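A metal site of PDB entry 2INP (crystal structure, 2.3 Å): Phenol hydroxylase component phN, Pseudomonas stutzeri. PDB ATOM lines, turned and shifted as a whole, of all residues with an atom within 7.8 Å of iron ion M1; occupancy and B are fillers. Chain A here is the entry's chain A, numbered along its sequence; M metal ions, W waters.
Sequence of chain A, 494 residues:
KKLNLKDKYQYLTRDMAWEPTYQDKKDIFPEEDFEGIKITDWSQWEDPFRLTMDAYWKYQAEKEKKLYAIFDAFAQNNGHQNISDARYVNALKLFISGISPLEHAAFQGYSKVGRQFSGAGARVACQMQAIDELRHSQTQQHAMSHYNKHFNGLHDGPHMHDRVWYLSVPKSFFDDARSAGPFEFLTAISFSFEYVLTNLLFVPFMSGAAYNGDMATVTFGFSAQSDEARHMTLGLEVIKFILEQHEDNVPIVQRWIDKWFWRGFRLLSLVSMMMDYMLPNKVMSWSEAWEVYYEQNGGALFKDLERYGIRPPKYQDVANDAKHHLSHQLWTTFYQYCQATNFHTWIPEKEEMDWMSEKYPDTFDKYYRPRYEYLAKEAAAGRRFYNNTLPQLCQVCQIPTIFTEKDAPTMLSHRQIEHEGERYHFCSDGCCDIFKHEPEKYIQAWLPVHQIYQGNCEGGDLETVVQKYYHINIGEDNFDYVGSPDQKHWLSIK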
ATOM      1  N   ILE A  99     -11.929  17.460 -12.665  1.00  0.00           N
ATOM      2  CA  ILE A  99     -12.102  16.437 -13.638  1.00  0.00           C
ATOM      3  C   ILE A  99     -13.554  16.277 -14.020  1.00  0.00           C
ATOM      4  O   ILE A  99     -13.892  16.164 -15.240  1.00  0.00           O
ATOM      5  CB  ILE A  99     -11.597  15.097 -13.113  1.00  0.00           C
ATOM      6  CG1 ILE A  99     -10.074  14.932 -13.137  1.00  0.00           C
ATOM      7  CG2 ILE A  99     -12.160  13.867 -13.957  1.00  0.00           C
ATOM      8  CD1 ILE A  99      -9.101  16.134 -13.325  1.00  0.00           C
ATOM      9  N   LEU A 102     -14.896  18.463 -16.516  1.00  0.00           N
ATOM     10  CA  LEU A 102     -14.493  18.037 -17.887  1.00  0.00           C
ATOM     11  C   LEU A 102     -15.468  16.997 -18.497  1.00  0.00           C
ATOM     12  O   LEU A 102     -15.654  16.968 -19.707  1.00  0.00           O
ATOM     13  CB  LEU A 102     -13.071  17.479 -17.874  1.00  0.00           C
ATOM     14  CG  LEU A 102     -11.814  18.309 -18.051  1.00  0.00           C
ATOM     15  CD1 LEU A 102     -11.989  19.833 -17.824  1.00  0.00           C
ATOM     16  CD2 LEU A 102     -10.651  17.623 -17.302  1.00  0.00           C
ATOM     17  N   GLU A 103     -16.092  16.167 -17.672  1.00  0.00           N
ATOM     18  CA  GLU A 103     -17.031  15.193 -18.163  1.00  0.00           C
ATOM     19  C   GLU A 103     -18.231  15.932 -18.721  1.00  0.00           C
ATOM     20  O   GLU A 103     -18.803  15.526 -19.730  1.00  0.00           O
ATOM     21  CB  GLU A 103     -17.553  14.319 -17.008  1.00  0.00           C
ATOM     22  CG  GLU A 103     -16.556  13.502 -16.196  1.00  0.00           C
ATOM     23  CD  GLU A 103     -15.982  12.312 -16.949  1.00  0.00           C
ATOM     24  OE1 GLU A 103     -15.158  11.529 -16.405  1.00  0.00           O
ATOM     25  OE2 GLU A 103     -16.348  12.132 -18.094  1.00  0.00           O
ATOM     26  N   HIS A 104     -18.670  16.983 -18.011  1.00  0.00           N
ATOM     27  CA  HIS A 104     -19.796  17.782 -18.482  1.00  0.00           C
ATOM     28  C   HIS A 104     -19.511  18.595 -19.741  1.00  0.00           C
ATOM     29  O   HIS A 104     -20.317  18.639 -20.611  1.00  0.00           O
ATOM     30  CB  HIS A 104     -20.371  18.644 -17.350  1.00  0.00           C
ATOM     31  CG  HIS A 104     -21.833  18.872 -17.485  1.00  0.00           C
ATOM     32  ND1 HIS A 104     -22.779  17.939 -17.076  1.00  0.00           N
ATOM     33  CD2 HIS A 104     -22.530  19.885 -18.072  1.00  0.00           C
ATOM     34  CE1 HIS A 104     -23.994  18.401 -17.345  1.00  0.00           C
ATOM     35  NE2 HIS A 104     -23.864  19.573 -17.960  1.00  0.00           N
ATOM     36  N   ALA A 106     -17.244  17.678 -22.058  1.00  0.00           N
ATOM     37  CA  ALA A 106     -17.255  16.606 -23.067  1.00  0.00           C
ATOM     38  C   ALA A 106     -18.667  16.206 -23.528  1.00  0.00           C
ATOM     39  O   ALA A 106     -18.894  16.060 -24.711  1.00  0.00           O
ATOM     40  CB  ALA A 106     -16.403  15.338 -22.604  1.00  0.00           C
ATOM     41  N   PHE A 107     -19.605  16.026 -22.623  1.00  0.00           N
ATOM     42  CA  PHE A 107     -20.975  15.903 -22.951  1.00  0.00           C
ATOM     43  C   PHE A 107     -21.425  16.994 -23.947  1.00  0.00           C
ATOM     44  O   PHE A 107     -22.006  16.692 -24.959  1.00  0.00           O
ATOM     45  CB  PHE A 107     -21.849  15.947 -21.672  1.00  0.00           C
ATOM     46  CG  PHE A 107     -23.274  16.367 -21.948  1.00  0.00           C
ATOM     47  CD1 PHE A 107     -24.065  15.674 -22.868  1.00  0.00           C
ATOM     48  CD2 PHE A 107     -23.835  17.478 -21.304  1.00  0.00           C
ATOM     49  CE1 PHE A 107     -25.427  16.102 -23.145  1.00  0.00           C
ATOM     50  CE2 PHE A 107     -25.133  17.904 -21.583  1.00  0.00           C
ATOM     51  CZ  PHE A 107     -25.915  17.210 -22.501  1.00  0.00           C
ATOM     52  N   TYR A 110     -19.245  16.674 -27.498  1.00  0.00           N
ATOM     53  CA  TYR A 110     -19.686  15.569 -28.324  1.00  0.00           C
ATOM     54  C   TYR A 110     -21.097  15.729 -28.819  1.00  0.00           C
ATOM     55  O   TYR A 110     -21.443  15.133 -29.842  1.00  0.00           O
ATOM     56  CB  TYR A 110     -19.544  14.208 -27.591  1.00  0.00           C
ATOM     57  CG  TYR A 110     -18.131  13.701 -27.528  1.00  0.00           C
ATOM     58  CD1 TYR A 110     -17.327  13.913 -26.372  1.00  0.00           C
ATOM     59  CD2 TYR A 110     -17.563  13.086 -28.621  1.00  0.00           C
ATOM     60  CE1 TYR A 110     -15.956  13.536 -26.337  1.00  0.00           C
ATOM     61  CE2 TYR A 110     -16.222  12.653 -28.607  1.00  0.00           C
ATOM     62  CZ  TYR A 110     -15.414  12.896 -27.454  1.00  0.00           C
ATOM     63  OH  TYR A 110     -14.081  12.467 -27.452  1.00  0.00           O
ATOM     64  N   GLN A 129     -21.255   8.735 -27.264  1.00  0.00           N
ATOM     65  CA  GLN A 129     -20.201   9.297 -26.398  1.00  0.00           C
ATOM     66  C   GLN A 129     -20.716  10.424 -25.503  1.00  0.00           C
ATOM     67  O   GLN A 129     -20.512  10.392 -24.300  1.00  0.00           O
ATOM     68  CB  GLN A 129     -19.028   9.750 -27.231  1.00  0.00           C
ATOM     69  CG  GLN A 129     -17.975  10.349 -26.347  1.00  0.00           C
ATOM     70  CD  GLN A 129     -16.672   9.607 -26.269  1.00  0.00           C
ATOM     71  OE1 GLN A 129     -16.367   8.734 -27.069  1.00  0.00           O
ATOM     72  NE2 GLN A 129     -15.860  10.010 -25.337  1.00  0.00           N
ATOM     73  N   ASP A 132     -22.951   9.339 -22.691  1.00  0.00           N
ATOM     74  CA  ASP A 132     -22.090   8.598 -21.777  1.00  0.00           C
ATOM     75  C   ASP A 132     -21.382   9.556 -20.838  1.00  0.00           C
ATOM     76  O   ASP A 132     -21.310   9.289 -19.659  1.00  0.00           O
ATOM     77  CB  ASP A 132     -20.986   7.854 -22.556  1.00  0.00           C
ATOM     78  CG  ASP A 132     -21.448   6.474 -23.104  1.00  0.00           C
ATOM     79  OD1 ASP A 132     -22.544   5.915 -22.737  1.00  0.00           O
ATOM     80  OD2 ASP A 132     -20.690   5.979 -23.978  1.00  0.00           O
ATOM     81  N   GLU A 133     -20.814  10.622 -21.418  1.00  0.00           N
ATOM     82  CA  GLU A 133     -20.168  11.731 -20.690  1.00  0.00           C
ATOM     83  C   GLU A 133     -21.089  12.362 -19.709  1.00  0.00           C
ATOM     84  O   GLU A 133     -20.644  12.747 -18.626  1.00  0.00           O
ATOM     85  CB  GLU A 133     -19.554  12.798 -21.618  1.00  0.00           C
ATOM     86  CG  GLU A 133     -18.604  12.229 -22.610  1.00  0.00           C
ATOM     87  CD  GLU A 133     -17.435  11.489 -21.901  1.00  0.00           C
ATOM     88  OE1 GLU A 133     -16.493  10.968 -22.545  1.00  0.00           O
ATOM     89  OE2 GLU A 133     -17.472  11.477 -20.649  1.00  0.00           O
ATOM     90  N   LEU A 134     -22.366  12.402 -20.051  1.00  0.00           N
ATOM     91  CA  LEU A 134     -23.339  12.994 -19.157  1.00  0.00           C
ATOM     92  C   LEU A 134     -23.645  12.037 -17.987  1.00  0.00           C
ATOM     93  O   LEU A 134     -23.770  12.474 -16.861  1.00  0.00           O
ATOM     94  CB  LEU A 134     -24.632  13.362 -19.926  1.00  0.00           C
ATOM     95  CG  LEU A 134     -25.818  13.878 -19.122  1.00  0.00           C
ATOM     96  CD1 LEU A 134     -25.583  15.275 -18.426  1.00  0.00           C
ATOM     97  CD2 LEU A 134     -27.115  13.889 -20.039  1.00  0.00           C
ATOM     98  N   ARG A 135     -23.802  10.746 -18.287  1.00  0.00           N
ATOM     99  CA  ARG A 135     -23.758   9.717 -17.272  1.00  0.00           C
ATOM    100  C   ARG A 135     -22.572   9.884 -16.309  1.00  0.00           C
ATOM    101  O   ARG A 135     -22.792   9.906 -15.137  1.00  0.00           O
ATOM    102  CB  ARG A 135     -23.643   8.346 -17.868  1.00  0.00           C
ATOM    103  CG  ARG A 135     -23.691   7.347 -16.736  1.00  0.00           C
ATOM    104  CD  ARG A 135     -23.893   5.990 -17.201  1.00  0.00           C
ATOM    105  NE  ARG A 135     -22.698   5.288 -17.094  1.00  0.00           N
ATOM    106  CZ  ARG A 135     -22.427   4.247 -16.300  1.00  0.00           C
ATOM    107  NH1 ARG A 135     -23.317   3.644 -15.488  1.00  0.00           N
ATOM    108  NH2 ARG A 135     -21.187   3.768 -16.389  1.00  0.00           N
ATOM    109  N   HIS A 136     -21.333  10.008 -16.817  1.00  0.00           N
ATOM    110  CA  HIS A 136     -20.188  10.199 -15.957  1.00  0.00           C
ATOM    111  C   HIS A 136     -20.302  11.437 -15.079  1.00  0.00           C
ATOM    112  O   HIS A 136     -19.980  11.376 -13.900  1.00  0.00           O
ATOM    113  CB  HIS A 136     -18.903  10.302 -16.754  1.00  0.00           C
ATOM    114  CG  HIS A 136     -18.633   9.082 -17.550  1.00  0.00           C
ATOM    115  ND1 HIS A 136     -17.604   8.966 -18.478  1.00  0.00           N
ATOM    116  CD2 HIS A 136     -19.298   7.902 -17.564  1.00  0.00           C
ATOM    117  CE1 HIS A 136     -17.648   7.761 -19.004  1.00  0.00           C
ATOM    118  NE2 HIS A 136     -18.677   7.107 -18.498  1.00  0.00           N
ATOM    119  N   SER A 137     -20.703  12.535 -15.687  1.00  0.00           N
ATOM    120  CA  SER A 137     -20.875  13.813 -15.031  1.00  0.00           C
ATOM    121  C   SER A 137     -21.875  13.647 -13.896  1.00  0.00           C
ATOM    122  O   SER A 137     -21.623  13.989 -12.773  1.00  0.00           O
ATOM    123  CB  SER A 137     -21.373  14.864 -16.018  1.00  0.00           C
ATOM    124  OG  SER A 137     -21.692  16.055 -15.317  1.00  0.00           O
ATOM    125  N   GLN A 140     -20.800  10.922 -11.079  1.00  0.00           N
ATOM    126  CA  GLN A 140     -19.795  11.509 -10.180  1.00  0.00           C
ATOM    127  C   GLN A 140     -20.374  12.458  -9.117  1.00  0.00           C
ATOM    128  O   GLN A 140     -19.919  12.452  -7.983  1.00  0.00           O
ATOM    129  CB  GLN A 140     -18.714  12.237 -10.995  1.00  0.00           C
ATOM    130  CG  GLN A 140     -17.940  11.188 -11.819  1.00  0.00           C
ATOM    131  CD  GLN A 140     -16.973  11.723 -12.856  1.00  0.00           C
ATOM    132  OE1 GLN A 140     -16.766  12.924 -12.953  1.00  0.00           O
ATOM    133  NE2 GLN A 140     -16.307  10.808 -13.620  1.00  0.00           N
ATOM    134  N   PHE A 193      -6.812  12.415 -25.492  1.00  0.00           N
ATOM    135  CA  PHE A 193      -7.247  12.347 -24.104  1.00  0.00           C
ATOM    136  C   PHE A 193      -7.816  10.957 -23.824  1.00  0.00           C
ATOM    137  O   PHE A 193      -7.396  10.314 -22.863  1.00  0.00           O
ATOM    138  CB  PHE A 193      -8.307  13.443 -23.921  1.00  0.00           C
ATOM    139  CG  PHE A 193      -8.731  13.714 -22.493  1.00  0.00           C
ATOM    140  CD1 PHE A 193      -7.853  14.332 -21.572  1.00  0.00           C
ATOM    141  CD2 PHE A 193     -10.066  13.463 -22.092  1.00  0.00           C
ATOM    142  CE1 PHE A 193      -8.289  14.690 -20.258  1.00  0.00           C
ATOM    143  CE2 PHE A 193     -10.518  13.789 -20.768  1.00  0.00           C
ATOM    144  CZ  PHE A 193      -9.625  14.429 -19.859  1.00  0.00           C
ATOM    145  N   GLU A 194      -8.728  10.455 -24.657  1.00  0.00           N
ATOM    146  CA  GLU A 194      -9.422   9.200 -24.366  1.00  0.00           C
ATOM    147  C   GLU A 194      -8.792   7.906 -24.835  1.00  0.00           C
ATOM    148  O   GLU A 194      -9.267   6.815 -24.487  1.00  0.00           O
ATOM    149  CB  GLU A 194     -10.864   9.269 -24.815  1.00  0.00           C
ATOM    150  CG  GLU A 194     -11.598  10.314 -24.023  1.00  0.00           C
ATOM    151  CD  GLU A 194     -12.872   9.878 -23.535  1.00  0.00           C
ATOM    152  OE1 GLU A 194     -13.679   9.340 -24.270  1.00  0.00           O
ATOM    153  OE2 GLU A 194     -13.110  10.043 -22.361  1.00  0.00           O
ATOM    154  N   LEU A 201      -5.109   9.125 -16.413  1.00  0.00           N
ATOM    155  CA  LEU A 201      -6.151   9.746 -15.598  1.00  0.00           C
ATOM    156  C   LEU A 201      -7.038   8.686 -14.846  1.00  0.00           C
ATOM    157  O   LEU A 201      -7.231   8.725 -13.619  1.00  0.00           O
ATOM    158  CB  LEU A 201      -6.985  10.660 -16.512  1.00  0.00           C
ATOM    159  CG  LEU A 201      -8.274  11.226 -15.919  1.00  0.00           C
ATOM    160  CD1 LEU A 201      -7.956  11.924 -14.608  1.00  0.00           C
ATOM    161  CD2 LEU A 201      -9.020  12.212 -16.898  1.00  0.00           C
ATOM    162  N   PHE A 202      -7.560   7.730 -15.591  1.00  0.00           N
ATOM    163  CA  PHE A 202      -8.511   6.811 -15.010  1.00  0.00           C
ATOM    164  C   PHE A 202      -7.821   6.007 -13.915  1.00  0.00           C
ATOM    165  O   PHE A 202      -8.221   6.088 -12.752  1.00  0.00           O
ATOM    166  CB  PHE A 202      -9.069   5.880 -16.101  1.00  0.00           C
ATOM    167  CG  PHE A 202     -10.435   5.216 -15.773  1.00  0.00           C
ATOM    168  CD1 PHE A 202     -10.482   3.852 -15.374  1.00  0.00           C
ATOM    169  CD2 PHE A 202     -11.650   5.937 -15.914  1.00  0.00           C
ATOM    170  CE1 PHE A 202     -11.745   3.217 -15.105  1.00  0.00           C
ATOM    171  CE2 PHE A 202     -12.933   5.351 -15.630  1.00  0.00           C
ATOM    172  CZ  PHE A 202     -12.980   3.977 -15.233  1.00  0.00           C
ATOM    173  N   PHE A 220     -17.883   3.502  -9.224  1.00  0.00           N
ATOM    174  CA  PHE A 220     -18.170   4.284 -10.426  1.00  0.00           C
ATOM    175  C   PHE A 220     -17.144   3.867 -11.523  1.00  0.00           C
ATOM    176  O   PHE A 220     -17.500   3.749 -12.717  1.00  0.00           O
ATOM    177  CB  PHE A 220     -18.095   5.808 -10.199  1.00  0.00           C
ATOM    178  CG  PHE A 220     -17.801   6.535 -11.483  1.00  0.00           C
ATOM    179  CD1 PHE A 220     -18.859   6.729 -12.483  1.00  0.00           C
ATOM    180  CD2 PHE A 220     -16.486   6.931 -11.796  1.00  0.00           C
ATOM    181  CE1 PHE A 220     -18.601   7.323 -13.720  1.00  0.00           C
ATOM    182  CE2 PHE A 220     -16.185   7.532 -13.115  1.00  0.00           C
ATOM    183  CZ  PHE A 220     -17.243   7.746 -14.068  1.00  0.00           C
ATOM    184  N   ALA A 224     -17.976   2.265 -15.343  1.00  0.00           N
ATOM    185  CA  ALA A 224     -17.635   3.114 -16.493  1.00  0.00           C
ATOM    186  C   ALA A 224     -16.672   2.434 -17.492  1.00  0.00           C
ATOM    187  O   ALA A 224     -16.444   2.994 -18.565  1.00  0.00           O
ATOM    188  CB  ALA A 224     -16.901   4.474 -15.995  1.00  0.00           C
ATOM    189  N   ASP A 227     -17.904   1.761 -20.901  1.00  0.00           N
ATOM    190  CA  ASP A 227     -18.108   3.010 -21.675  1.00  0.00           C
ATOM    191  C   ASP A 227     -16.780   3.470 -22.237  1.00  0.00           C
ATOM    192  O   ASP A 227     -16.672   3.819 -23.399  1.00  0.00           O
ATOM    193  CB  ASP A 227     -18.594   4.170 -20.796  1.00  0.00           C
ATOM    194  CG  ASP A 227     -19.920   3.880 -20.071  1.00  0.00           C
ATOM    195  OD1 ASP A 227     -20.673   3.031 -20.512  1.00  0.00           O
ATOM    196  OD2 ASP A 227     -20.157   4.498 -19.006  1.00  0.00           O
ATOM    197  N   GLU A 228     -15.762   3.487 -21.398  1.00  0.00           N
ATOM    198  CA  GLU A 228     -14.482   3.900 -21.877  1.00  0.00           C
ATOM    199  C   GLU A 228     -13.933   2.950 -22.981  1.00  0.00           C
ATOM    200  O   GLU A 228     -13.303   3.446 -23.872  1.00  0.00           O
ATOM    201  CB  GLU A 228     -13.492   4.121 -20.749  1.00  0.00           C
ATOM    202  CG  GLU A 228     -13.805   5.411 -19.888  1.00  0.00           C
ATOM    203  CD  GLU A 228     -14.118   6.685 -20.710  1.00  0.00           C
ATOM    204  OE1 GLU A 228     -13.403   7.129 -21.661  1.00  0.00           O
ATOM    205  OE2 GLU A 228     -15.136   7.303 -20.357  1.00  0.00           O
ATOM    206  N   HIS A 231     -15.258   4.420 -26.055  1.00  0.00           N
ATOM    207  CA  HIS A 231     -14.655   5.699 -26.347  1.00  0.00           C
ATOM    208  C   HIS A 231     -13.253   5.572 -26.858  1.00  0.00           C
ATOM    209  O   HIS A 231     -12.822   6.406 -27.622  1.00  0.00           O
ATOM    210  CB  HIS A 231     -14.685   6.582 -25.070  1.00  0.00           C
ATOM    211  CG  HIS A 231     -16.068   6.701 -24.480  1.00  0.00           C
ATOM    212  ND1 HIS A 231     -16.313   7.174 -23.213  1.00  0.00           N
ATOM    213  CD2 HIS A 231     -17.299   6.408 -24.993  1.00  0.00           C
ATOM    214  CE1 HIS A 231     -17.613   7.179 -22.962  1.00  0.00           C
ATOM    215  NE2 HIS A 231     -18.230   6.704 -24.020  1.00  0.00           N
HETATM  216 FE    FE M   1     -16.024  10.403 -19.340  1.00  0.00          FE
HETATM  217 FE    FE M   2     -14.819   8.689 -21.904  1.00  0.00          FE
HETATM  218  O   HOH W   1     -14.586   9.385 -17.151  1.00  0.00           O
HETATM  219  O   HOH W   2     -14.608  11.583 -19.888  1.00  0.00           O
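Glu 228 touches iron ion M1.
Of the 24 residues printed, 4 come within 4 Å of iron ion M1.
Along chain A the residues within 4 Å of iron ion M1 span positions 103 to 228.
The side-chain carboxylate (OE1) of Glu 103 sits at hydrogen-bond distance from the side-chain amide nitrogen (NE2) of Gln 140.
The side-chain carboxylate (OE1) of Glu 133 lies within hydrogen-bond range of the side-chain amide nitrogen (NE2) of Gln 129 (3.0 Å).
A ring nitrogen (NE2) of His 136 lies within hydrogen-bond range of the side-chain carboxylate (OD2) of Asp 227 (3.0 Å).
Iron ion M1 is bound by water W2 (1.9 Å), the side-chain carboxylate of Glu 103 (2.2 Å), the side-chain carboxylate of Glu 133 (2.2 Å) and a ring nitrogen (ND1) of His 136 (2.3 Å).
Slightly farther from iron ion M1 lies water W1 (2.8 Å).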
